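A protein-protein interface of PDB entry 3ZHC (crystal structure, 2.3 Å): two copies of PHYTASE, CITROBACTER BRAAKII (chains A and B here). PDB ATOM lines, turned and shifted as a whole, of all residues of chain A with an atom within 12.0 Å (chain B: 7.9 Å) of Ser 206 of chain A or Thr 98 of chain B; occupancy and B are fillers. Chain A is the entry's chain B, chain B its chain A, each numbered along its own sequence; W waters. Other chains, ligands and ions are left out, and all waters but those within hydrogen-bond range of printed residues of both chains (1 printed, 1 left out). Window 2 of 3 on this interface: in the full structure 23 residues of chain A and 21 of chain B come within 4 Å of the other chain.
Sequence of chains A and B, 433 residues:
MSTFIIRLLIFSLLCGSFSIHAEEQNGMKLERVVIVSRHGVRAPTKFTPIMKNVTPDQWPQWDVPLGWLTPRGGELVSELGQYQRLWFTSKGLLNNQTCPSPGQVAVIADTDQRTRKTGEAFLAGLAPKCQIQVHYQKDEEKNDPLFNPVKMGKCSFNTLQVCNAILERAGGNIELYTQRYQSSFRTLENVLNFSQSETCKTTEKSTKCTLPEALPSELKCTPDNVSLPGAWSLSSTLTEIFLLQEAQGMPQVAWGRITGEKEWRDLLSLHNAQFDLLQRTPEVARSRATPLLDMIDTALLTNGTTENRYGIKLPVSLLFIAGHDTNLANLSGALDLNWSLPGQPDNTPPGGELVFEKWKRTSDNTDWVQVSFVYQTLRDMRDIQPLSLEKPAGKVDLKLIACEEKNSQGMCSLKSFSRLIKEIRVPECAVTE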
ATOM      1  N   GLN A 182     -17.985 -22.355  -7.147  1.00  0.00           N
ATOM      2  CA  GLN A 182     -19.217 -22.657  -7.960  1.00  0.00           C
ATOM      3  C   GLN A 182     -19.393 -21.749  -9.158  1.00  0.00           C
ATOM      4  O   GLN A 182     -19.490 -22.222 -10.277  1.00  0.00           O
ATOM      5  CB  GLN A 182     -20.508 -22.552  -7.127  1.00  0.00           C
ATOM      6  CG  GLN A 182     -20.783 -23.716  -6.279  1.00  0.00           C
ATOM      7  CD  GLN A 182     -22.139 -23.631  -5.551  1.00  0.00           C
ATOM      8  OE1 GLN A 182     -22.197 -23.687  -4.299  1.00  0.00           O
ATOM      9  NE2 GLN A 182     -23.242 -23.494  -6.330  1.00  0.00           N
ATOM     10  N   ARG A 186     -19.563 -22.185 -13.287  1.00  0.00           N
ATOM     11  CA  ARG A 186     -20.690 -21.711 -14.119  1.00  0.00           C
ATOM     12  C   ARG A 186     -20.183 -20.914 -15.323  1.00  0.00           C
ATOM     13  O   ARG A 186     -20.717 -21.058 -16.433  1.00  0.00           O
ATOM     14  CB  ARG A 186     -21.695 -20.830 -13.324  1.00  0.00           C
ATOM     15  CG  ARG A 186     -22.406 -21.488 -12.114  1.00  0.00           C
ATOM     16  CD  ARG A 186     -23.190 -22.759 -12.491  1.00  0.00           C
ATOM     17  NE  ARG A 186     -22.317 -23.921 -12.527  1.00  0.00           N
ATOM     18  CZ  ARG A 186     -21.919 -24.630 -11.447  1.00  0.00           C
ATOM     19  NH1 ARG A 186     -22.319 -24.316 -10.208  1.00  0.00           N
ATOM     20  NH2 ARG A 186     -21.106 -25.673 -11.619  1.00  0.00           N
ATOM     21  N   GLU A 189     -18.528 -23.350 -17.815  1.00  0.00           N
ATOM     22  CA  GLU A 189     -19.670 -24.044 -18.458  1.00  0.00           C
ATOM     23  C   GLU A 189     -20.364 -23.191 -19.525  1.00  0.00           C
ATOM     24  O   GLU A 189     -20.693 -23.701 -20.587  1.00  0.00           O
ATOM     25  CB  GLU A 189     -20.665 -24.485 -17.406  1.00  0.00           C
ATOM     26  CG  GLU A 189     -20.155 -25.678 -16.559  1.00  0.00           C
ATOM     27  CD  GLU A 189     -20.856 -25.810 -15.217  1.00  0.00           C
ATOM     28  OE1 GLU A 189     -21.918 -25.167 -15.010  1.00  0.00           O
ATOM     29  OE2 GLU A 189     -20.345 -26.557 -14.351  1.00  0.00           O
ATOM     30  N   SER A 195     -23.908 -27.310 -21.333  1.00  0.00           N
ATOM     31  CA  SER A 195     -25.276 -27.889 -21.333  1.00  0.00           C
ATOM     32  C   SER A 195     -25.664 -28.559 -22.659  1.00  0.00           C
ATOM     33  O   SER A 195     -26.443 -29.505 -22.673  1.00  0.00           O
ATOM     34  CB  SER A 195     -26.322 -26.806 -21.001  1.00  0.00           C
ATOM     35  OG  SER A 195     -26.148 -26.312 -19.689  1.00  0.00           O
ATOM     36  N   CYS A 200     -23.524 -33.768 -21.385  1.00  0.00           N
ATOM     37  CA  CYS A 200     -24.889 -33.491 -20.850  1.00  0.00           C
ATOM     38  C   CYS A 200     -26.036 -34.034 -21.730  1.00  0.00           C
ATOM     39  O   CYS A 200     -27.204 -33.663 -21.528  1.00  0.00           O
ATOM     40  CB  CYS A 200     -25.068 -31.978 -20.669  1.00  0.00           C
ATOM     41  SG  CYS A 200     -23.890 -31.276 -19.538  1.00  0.00           S
ATOM     42  N   THR A 202     -27.451 -37.155 -22.063  1.00  0.00           N
ATOM     43  CA  THR A 202     -28.416 -38.022 -21.341  1.00  0.00           C
ATOM     44  C   THR A 202     -29.023 -37.401 -20.066  1.00  0.00           C
ATOM     45  O   THR A 202     -30.180 -37.683 -19.731  1.00  0.00           O
ATOM     46  CB  THR A 202     -27.763 -39.389 -20.944  1.00  0.00           C
ATOM     47  OG1 THR A 202     -26.747 -39.182 -19.950  1.00  0.00           O
ATOM     48  CG2 THR A 202     -27.153 -40.091 -22.175  1.00  0.00           C
ATOM     49  N   THR A 203     -28.244 -36.565 -19.365  1.00  0.00           N
ATOM     50  CA  THR A 203     -28.674 -35.985 -18.071  1.00  0.00           C
ATOM     51  C   THR A 203     -29.691 -34.835 -18.237  1.00  0.00           C
ATOM     52  O   THR A 203     -29.431 -33.865 -18.958  1.00  0.00           O
ATOM     53  CB  THR A 203     -27.460 -35.504 -17.219  1.00  0.00           C
ATOM     54  OG1 THR A 203     -26.818 -34.399 -17.858  1.00  0.00           O
ATOM     55  CG2 THR A 203     -26.452 -36.661 -17.010  1.00  0.00           C
ATOM     56  N   GLU A 204     -30.842 -34.979 -17.559  1.00  0.00           N
ATOM     57  CA  GLU A 204     -31.933 -33.988 -17.555  1.00  0.00           C
ATOM     58  C   GLU A 204     -32.466 -33.833 -16.122  1.00  0.00           C
ATOM     59  O   GLU A 204     -32.976 -34.807 -15.546  1.00  0.00           O
ATOM     60  CB  GLU A 204     -33.071 -34.424 -18.490  1.00  0.00           C
ATOM     61  CG  GLU A 204     -32.656 -34.675 -19.975  1.00  0.00           C
ATOM     62  CD  GLU A 204     -32.115 -33.417 -20.696  1.00  0.00           C
ATOM     63  OE1 GLU A 204     -32.445 -32.276 -20.268  1.00  0.00           O
ATOM     64  OE2 GLU A 204     -31.350 -33.579 -21.701  1.00  0.00           O
ATOM     65  N   LYS A 205     -32.345 -32.629 -15.548  1.00  0.00           N
ATOM     66  CA  LYS A 205     -32.804 -32.362 -14.157  1.00  0.00           C
ATOM     67  C   LYS A 205     -33.200 -30.883 -13.926  1.00  0.00           C
ATOM     68  O   LYS A 205     -32.988 -30.023 -14.810  1.00  0.00           O
ATOM     69  CB  LYS A 205     -31.734 -32.823 -13.145  1.00  0.00           C
ATOM     70  CG  LYS A 205     -30.374 -32.110 -13.263  1.00  0.00           C
ATOM     71  CD  LYS A 205     -29.262 -32.930 -12.589  1.00  0.00           C
ATOM     72  CE  LYS A 205     -27.893 -32.263 -12.757  1.00  0.00           C
ATOM     73  NZ  LYS A 205     -26.765 -33.141 -12.336  1.00  0.00           N
ATOM     74  N   SER A 206     -33.779 -30.615 -12.743  1.00  0.00           N
ATOM     75  CA  SER A 206     -34.262 -29.255 -12.340  1.00  0.00           C
ATOM     76  C   SER A 206     -33.152 -28.211 -12.389  1.00  0.00           C
ATOM     77  O   SER A 206     -33.314 -27.122 -12.954  1.00  0.00           O
ATOM     78  CB  SER A 206     -34.854 -29.297 -10.923  1.00  0.00           C
ATOM     79  OG  SER A 206     -35.804 -30.356 -10.789  1.00  0.00           O
ATOM     80  N   THR A 207     -32.025 -28.568 -11.784  1.00  0.00           N
ATOM     81  CA  THR A 207     -30.832 -27.759 -11.800  1.00  0.00           C
ATOM     82  C   THR A 207     -30.069 -27.961 -13.130  1.00  0.00           C
ATOM     83  O   THR A 207     -30.456 -28.771 -13.977  1.00  0.00           O
ATOM     84  CB  THR A 207     -29.925 -28.120 -10.611  1.00  0.00           C
ATOM     85  OG1 THR A 207     -29.692 -29.535 -10.596  1.00  0.00           O
ATOM     86  CG2 THR A 207     -30.573 -27.693  -9.278  1.00  0.00           C
ATOM     87  N   LYS A 208     -28.994 -27.212 -13.295  1.00  0.00           N
ATOM     88  CA  LYS A 208     -28.091 -27.345 -14.451  1.00  0.00           C
ATOM     89  C   LYS A 208     -27.322 -28.645 -14.510  1.00  0.00           C
ATOM     90  O   LYS A 208     -27.074 -29.285 -13.483  1.00  0.00           O
ATOM     91  CB  LYS A 208     -27.027 -26.217 -14.412  1.00  0.00           C
ATOM     92  CG  LYS A 208     -27.271 -25.055 -15.331  1.00  0.00           C
ATOM     93  CD  LYS A 208     -26.297 -25.044 -16.495  1.00  0.00           C
ATOM     94  CE  LYS A 208     -24.934 -24.530 -16.030  1.00  0.00           C
ATOM     95  NZ  LYS A 208     -23.879 -24.988 -16.908  1.00  0.00           N
ATOM     96  N   CYS A 209     -26.941 -29.024 -15.729  1.00  0.00           N
ATOM     97  CA  CYS A 209     -25.920 -30.028 -15.935  1.00  0.00           C
ATOM     98  C   CYS A 209     -24.603 -29.274 -15.598  1.00  0.00           C
ATOM     99  O   CYS A 209     -24.353 -28.215 -16.163  1.00  0.00           O
ATOM    100  CB  CYS A 209     -25.913 -30.534 -17.365  1.00  0.00           C
ATOM    101  SG  CYS A 209     -24.663 -31.780 -17.698  1.00  0.00           S
ATOM    102  N   THR A 210     -23.795 -29.809 -14.679  1.00  0.00           N
ATOM    103  CA  THR A 210     -22.534 -29.139 -14.256  1.00  0.00           C
ATOM    104  C   THR A 210     -21.300 -30.036 -14.405  1.00  0.00           C
ATOM    105  O   THR A 210     -21.403 -31.264 -14.402  1.00  0.00           O
ATOM    106  CB  THR A 210     -22.621 -28.615 -12.798  1.00  0.00           C
ATOM    107  OG1 THR A 210     -22.758 -29.712 -11.901  1.00  0.00           O
ATOM    108  CG2 THR A 210     -23.795 -27.648 -12.627  1.00  0.00           C
ATOM    109  N   GLU A 213     -20.332 -32.210 -11.131  1.00  0.00           N
ATOM    110  CA  GLU A 213     -21.271 -33.338 -10.974  1.00  0.00           C
ATOM    111  C   GLU A 213     -21.014 -34.401 -12.058  1.00  0.00           C
ATOM    112  O   GLU A 213     -21.068 -35.587 -11.774  1.00  0.00           O
ATOM    113  CB  GLU A 213     -22.741 -32.841 -10.998  1.00  0.00           C
ATOM    114  CG  GLU A 213     -23.802 -33.858 -10.425  1.00  0.00           C
ATOM    115  CD  GLU A 213     -23.811 -33.984  -8.854  1.00  0.00           C
ATOM    116  OE1 GLU A 213     -23.170 -33.159  -8.150  1.00  0.00           O
ATOM    117  OE2 GLU A 213     -24.480 -34.928  -8.341  1.00  0.00           O
ATOM    118  N   ARG B  85     -32.229 -18.859   2.374  1.00  0.00           N
ATOM    119  CA  ARG B  85     -33.094 -19.879   1.721  1.00  0.00           C
ATOM    120  C   ARG B  85     -33.885 -20.638   2.789  1.00  0.00           C
ATOM    121  O   ARG B  85     -35.093 -20.770   2.677  1.00  0.00           O
ATOM    122  CB  ARG B  85     -32.291 -20.871   0.810  1.00  0.00           C
ATOM    123  CG  ARG B  85     -32.980 -22.299   0.618  1.00  0.00           C
ATOM    124  CD  ARG B  85     -32.525 -23.095  -0.618  1.00  0.00           C
ATOM    125  NE  ARG B  85     -33.284 -22.693  -1.831  1.00  0.00           N
ATOM    126  CZ  ARG B  85     -33.436 -23.430  -2.958  1.00  0.00           C
ATOM    127  NH1 ARG B  85     -32.890 -24.657  -3.091  1.00  0.00           N
ATOM    128  NH2 ARG B  85     -34.153 -22.924  -3.974  1.00  0.00           N
ATOM    129  N   ASN B  95     -40.978 -20.907  -1.923  1.00  0.00           N
ATOM    130  CA  ASN B  95     -41.571 -22.268  -1.826  1.00  0.00           C
ATOM    131  C   ASN B  95     -40.497 -23.313  -1.545  1.00  0.00           C
ATOM    132  O   ASN B  95     -39.351 -23.161  -2.012  1.00  0.00           O
ATOM    133  CB  ASN B  95     -42.330 -22.626  -3.116  1.00  0.00           C
ATOM    134  CG  ASN B  95     -43.349 -21.547  -3.532  1.00  0.00           C
ATOM    135  OD1 ASN B  95     -43.832 -20.772  -2.701  1.00  0.00           O
ATOM    136  ND2 ASN B  95     -43.665 -21.500  -4.820  1.00  0.00           N
ATOM    137  N   ASN B  96     -40.844 -24.372  -0.784  1.00  0.00           N
ATOM    138  CA  ASN B  96     -39.890 -25.480  -0.513  1.00  0.00           C
ATOM    139  C   ASN B  96     -39.727 -26.242  -1.838  1.00  0.00           C
ATOM    140  O   ASN B  96     -40.484 -27.179  -2.145  1.00  0.00           O
ATOM    141  CB  ASN B  96     -40.343 -26.379   0.653  1.00  0.00           C
ATOM    142  CG  ASN B  96     -39.180 -27.235   1.243  1.00  0.00           C
ATOM    143  OD1 ASN B  96     -38.174 -27.510   0.571  1.00  0.00           O
ATOM    144  ND2 ASN B  96     -39.332 -27.644   2.504  1.00  0.00           N
ATOM    145  N   GLN B  97     -38.728 -25.804  -2.613  1.00  0.00           N
ATOM    146  CA  GLN B  97     -38.553 -26.205  -3.998  1.00  0.00           C
ATOM    147  C   GLN B  97     -37.077 -26.122  -4.412  1.00  0.00           C
ATOM    148  O   GLN B  97     -36.281 -25.413  -3.767  1.00  0.00           O
ATOM    149  CB  GLN B  97     -39.406 -25.250  -4.827  1.00  0.00           C
ATOM    150  CG  GLN B  97     -39.587 -25.557  -6.282  1.00  0.00           C
ATOM    151  CD  GLN B  97     -40.474 -24.510  -6.984  1.00  0.00           C
ATOM    152  OE1 GLN B  97     -41.039 -23.603  -6.341  1.00  0.00           O
ATOM    153  NE2 GLN B  97     -40.598 -24.635  -8.305  1.00  0.00           N
ATOM    154  N   THR B  98     -36.714 -26.846  -5.485  1.00  0.00           N
ATOM    155  CA  THR B  98     -35.316 -26.897  -5.977  1.00  0.00           C
ATOM    156  C   THR B  98     -34.850 -25.514  -6.478  1.00  0.00           C
ATOM    157  O   THR B  98     -33.825 -24.993  -6.001  1.00  0.00           O
ATOM    158  CB  THR B  98     -35.120 -27.990  -7.079  1.00  0.00           C
ATOM    159  OG1 THR B  98     -35.533 -29.267  -6.568  1.00  0.00           O
ATOM    160  CG2 THR B  98     -33.659 -28.079  -7.524  1.00  0.00           C
ATOM    161  N   CYS B  99     -35.608 -24.937  -7.423  1.00  0.00           N
ATOM    162  CA  CYS B  99     -35.341 -23.588  -7.956  1.00  0.00           C
ATOM    163  C   CYS B  99     -36.565 -22.692  -7.802  1.00  0.00           C
ATOM    164  O   CYS B  99     -37.696 -23.191  -7.842  1.00  0.00           O
ATOM    165  CB  CYS B  99     -34.923 -23.649  -9.422  1.00  0.00           C
ATOM    166  SG  CYS B  99     -33.275 -24.278  -9.689  1.00  0.00           S
ATOM    167  N   PRO B 100     -36.352 -21.350  -7.630  1.00  0.00           N
ATOM    168  CA  PRO B 100     -37.518 -20.477  -7.451  1.00  0.00           C
ATOM    169  C   PRO B 100     -38.305 -20.301  -8.734  1.00  0.00           C
ATOM    170  O   PRO B 100     -37.734 -20.418  -9.832  1.00  0.00           O
ATOM    171  CB  PRO B 100     -36.897 -19.129  -7.012  1.00  0.00           C
ATOM    172  CG  PRO B 100     -35.433 -19.375  -6.862  1.00  0.00           C
ATOM    173  CD  PRO B 100     -35.098 -20.570  -7.654  1.00  0.00           C
ATOM    174  N   SER B 101     -39.607 -20.021  -8.595  1.00  0.00           N
ATOM    175  CA  SER B 101     -40.484 -19.776  -9.752  1.00  0.00           C
ATOM    176  C   SER B 101     -40.130 -18.428 -10.413  1.00  0.00           C
ATOM    177  O   SER B 101     -39.480 -17.593  -9.776  1.00  0.00           O
ATOM    178  CB  SER B 101     -41.958 -19.782  -9.333  1.00  0.00           C
ATOM    179  OG  SER B 101     -42.322 -21.032  -8.777  1.00  0.00           O
ATOM    180  N   LEU B 126     -28.418 -19.424  -2.133  1.00  0.00           N
ATOM    181  CA  LEU B 126     -29.882 -19.321  -2.195  1.00  0.00           C
ATOM    182  C   LEU B 126     -30.503 -20.319  -3.179  1.00  0.00           C
ATOM    183  O   LEU B 126     -31.419 -21.052  -2.819  1.00  0.00           O
ATOM    184  CB  LEU B 126     -30.317 -17.907  -2.606  1.00  0.00           C
ATOM    185  CG  LEU B 126     -31.823 -17.594  -2.451  1.00  0.00           C
ATOM    186  CD1 LEU B 126     -32.132 -17.184  -1.005  1.00  0.00           C
ATOM    187  CD2 LEU B 126     -32.253 -16.515  -3.407  1.00  0.00           C
ATOM    188  N   ALA B 127     -29.999 -20.318  -4.420  1.00  0.00           N
ATOM    189  CA  ALA B 127     -30.538 -21.150  -5.514  1.00  0.00           C
ATOM    190  C   ALA B 127     -29.400 -21.744  -6.334  1.00  0.00           C
ATOM    191  O   ALA B 127     -29.167 -21.322  -7.481  1.00  0.00           O
ATOM    192  CB  ALA B 127     -31.460 -20.315  -6.387  1.00  0.00           C
ATOM    193  N   PRO B 128     -28.665 -22.721  -5.750  1.00  0.00           N
ATOM    194  CA  PRO B 128     -27.516 -23.286  -6.462  1.00  0.00           C
ATOM    195  C   PRO B 128     -27.913 -23.911  -7.789  1.00  0.00           C
ATOM    196  O   PRO B 128     -28.863 -24.687  -7.832  1.00  0.00           O
ATOM    197  CB  PRO B 128     -26.968 -24.353  -5.492  1.00  0.00           C
ATOM    198  CG  PRO B 128     -27.988 -24.532  -4.456  1.00  0.00           C
ATOM    199  CD  PRO B 128     -28.838 -23.319  -4.414  1.00  0.00           C
ATOM    200  N   LYS B 129     -27.185 -23.535  -8.853  1.00  0.00           N
ATOM    201  CA  LYS B 129     -27.351 -24.078 -10.216  1.00  0.00           C
ATOM    202  C   LYS B 129     -28.703 -23.709 -10.904  1.00  0.00           C
ATOM    203  O   LYS B 129     -29.068 -24.331 -11.910  1.00  0.00           O
ATOM    204  CB  LYS B 129     -27.122 -25.604 -10.212  1.00  0.00           C
ATOM    205  CG  LYS B 129     -25.811 -26.033  -9.536  1.00  0.00           C
ATOM    206  CD  LYS B 129     -25.771 -27.500  -9.289  1.00  0.00           C
ATOM    207  CE  LYS B 129     -24.552 -27.863  -8.478  1.00  0.00           C
ATOM    208  NZ  LYS B 129     -24.463 -29.349  -8.264  1.00  0.00           N
ATOM    209  N   CYS B 130     -29.420 -22.700 -10.369  1.00  0.00           N
ATOM    210  CA  CYS B 130     -30.734 -22.267 -10.929  1.00  0.00           C
ATOM    211  C   CYS B 130     -30.615 -21.241 -12.050  1.00  0.00           C
ATOM    212  O   CYS B 130     -31.616 -20.907 -12.663  1.00  0.00           O
ATOM    213  CB  CYS B 130     -31.650 -21.731  -9.812  1.00  0.00           C
ATOM    214  SG  CYS B 130     -32.087 -22.988  -8.612  1.00  0.00           S
ATOM    215  N   GLN B 131     -29.387 -20.750 -12.303  1.00  0.00           N
ATOM    216  CA  GLN B 131     -29.080 -19.794 -13.407  1.00  0.00           C
ATOM    217  C   GLN B 131     -29.820 -18.426 -13.298  1.00  0.00           C
ATOM    218  O   GLN B 131     -30.124 -17.777 -14.329  1.00  0.00           O
ATOM    219  CB  GLN B 131     -29.332 -20.447 -14.782  1.00  0.00           C
ATOM    220  CG  GLN B 131     -28.675 -21.816 -14.962  1.00  0.00           C
ATOM    221  CD  GLN B 131     -28.865 -22.368 -16.370  1.00  0.00           C
ATOM    222  OE1 GLN B 131     -29.756 -23.183 -16.607  1.00  0.00           O
ATOM    223  NE2 GLN B 131     -28.031 -21.917 -17.310  1.00  0.00           N
HETATM  224  O   HOH W   1     -21.699 -29.076  -9.371  1.00  0.00           O
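Water W1 lies within hydrogen-bond range of OG1 of Thr 210 of chain A and NZ of Lys 129 of chain B.
Gln 182 of chain A touches Pro 128 of chain B (NE2 to CB, 3.9 Å). Lys 129 of chain B touches Arg 186 of chain A (CG to NH1, 3.9 Å). Thr 98 of chain B touches Ser 206 of chain A (CG2 to CB, 3.8 Å). CG2 of Thr 98 of chain B touches CG2 of Thr 207 of chain A, 3.6 Å away. Pro 128 of chain B touches Thr 207 of chain A (O to CG2, 3.7 Å). Lys 129 of chain B touches Thr 207 of chain A. Gln 131 of chain B touches Lys 208 of chain A (CD to CG, 3.3 Å). CG2 of Thr 210 of chain A touches CD of Lys 129 of chain B (3.9 Å).
The guanidinium group (NE) of Arg 186 of chain A lies within salt-bridge range of the side-chain carboxylate (OE1) of Glu 189 of chain A (2.8 Å). The side-chain sulfur (SG) of Cys 99 of chain B is disulfide-bonded to the side-chain sulfur (SG) of Cys 130 of chain B (2.1 Å). The side-chain amino group (NZ) of Lys 208 of chain A is in salt-bridge range of the side-chain carboxylate (OE1) of Glu 189 of chain A. The guanidinium group (NH2) of Arg 85 of chain B sits at hydrogen-bond distance from the backbone carbonyl oxygen (O) of Thr 98 of chain B, 2.9 Å away. The side-chain sulfur of Cys 200 of chain A is disulfide-bonded to the side-chain sulfur of Cys 209 of chain A.
No position is printed for both chains.
Along chain B the printed residues that touch a printed residue of chain A span positions 98 to 131. Among the printed residues, 9 pairs touch across the chains.
N of Lys 208 of chain A is in hydrogen-bond range of O of Lys 129 of chain B (3.2 Å).
Thr 203 of chain A touches none of the printed residues of chain B. Ser 206 of chain A touches just one residue of chain B: Thr 98. Printed residues of chain B within 4 Å of Lys 208 of chain A: Lys 129 (3.2 Å) and Gln 131 (3.3 Å). Printed residues of chain B within 4 Å of Thr 210 of chain A: Lys 129 (3.9 Å). Arg 85 of chain B touches none of the printed residues of chain A. Printed residues of chain A within 4 Å of Thr 98 of chain B: Ser 206 and Thr 207. No residue of chain A comes within 4 Å of Cys 99 of chain B. No residue of chain A comes within 4 Å of Pro 100 of chain B. Ala 127 of chain B touches none of the printed residues of chain A. No residue of chain A comes within 4 Å of Cys 130 of chain B. The nearest residue of chain B that does not touch Ser 206 of chain A is Cys 99 of chain B (4.3 Å).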
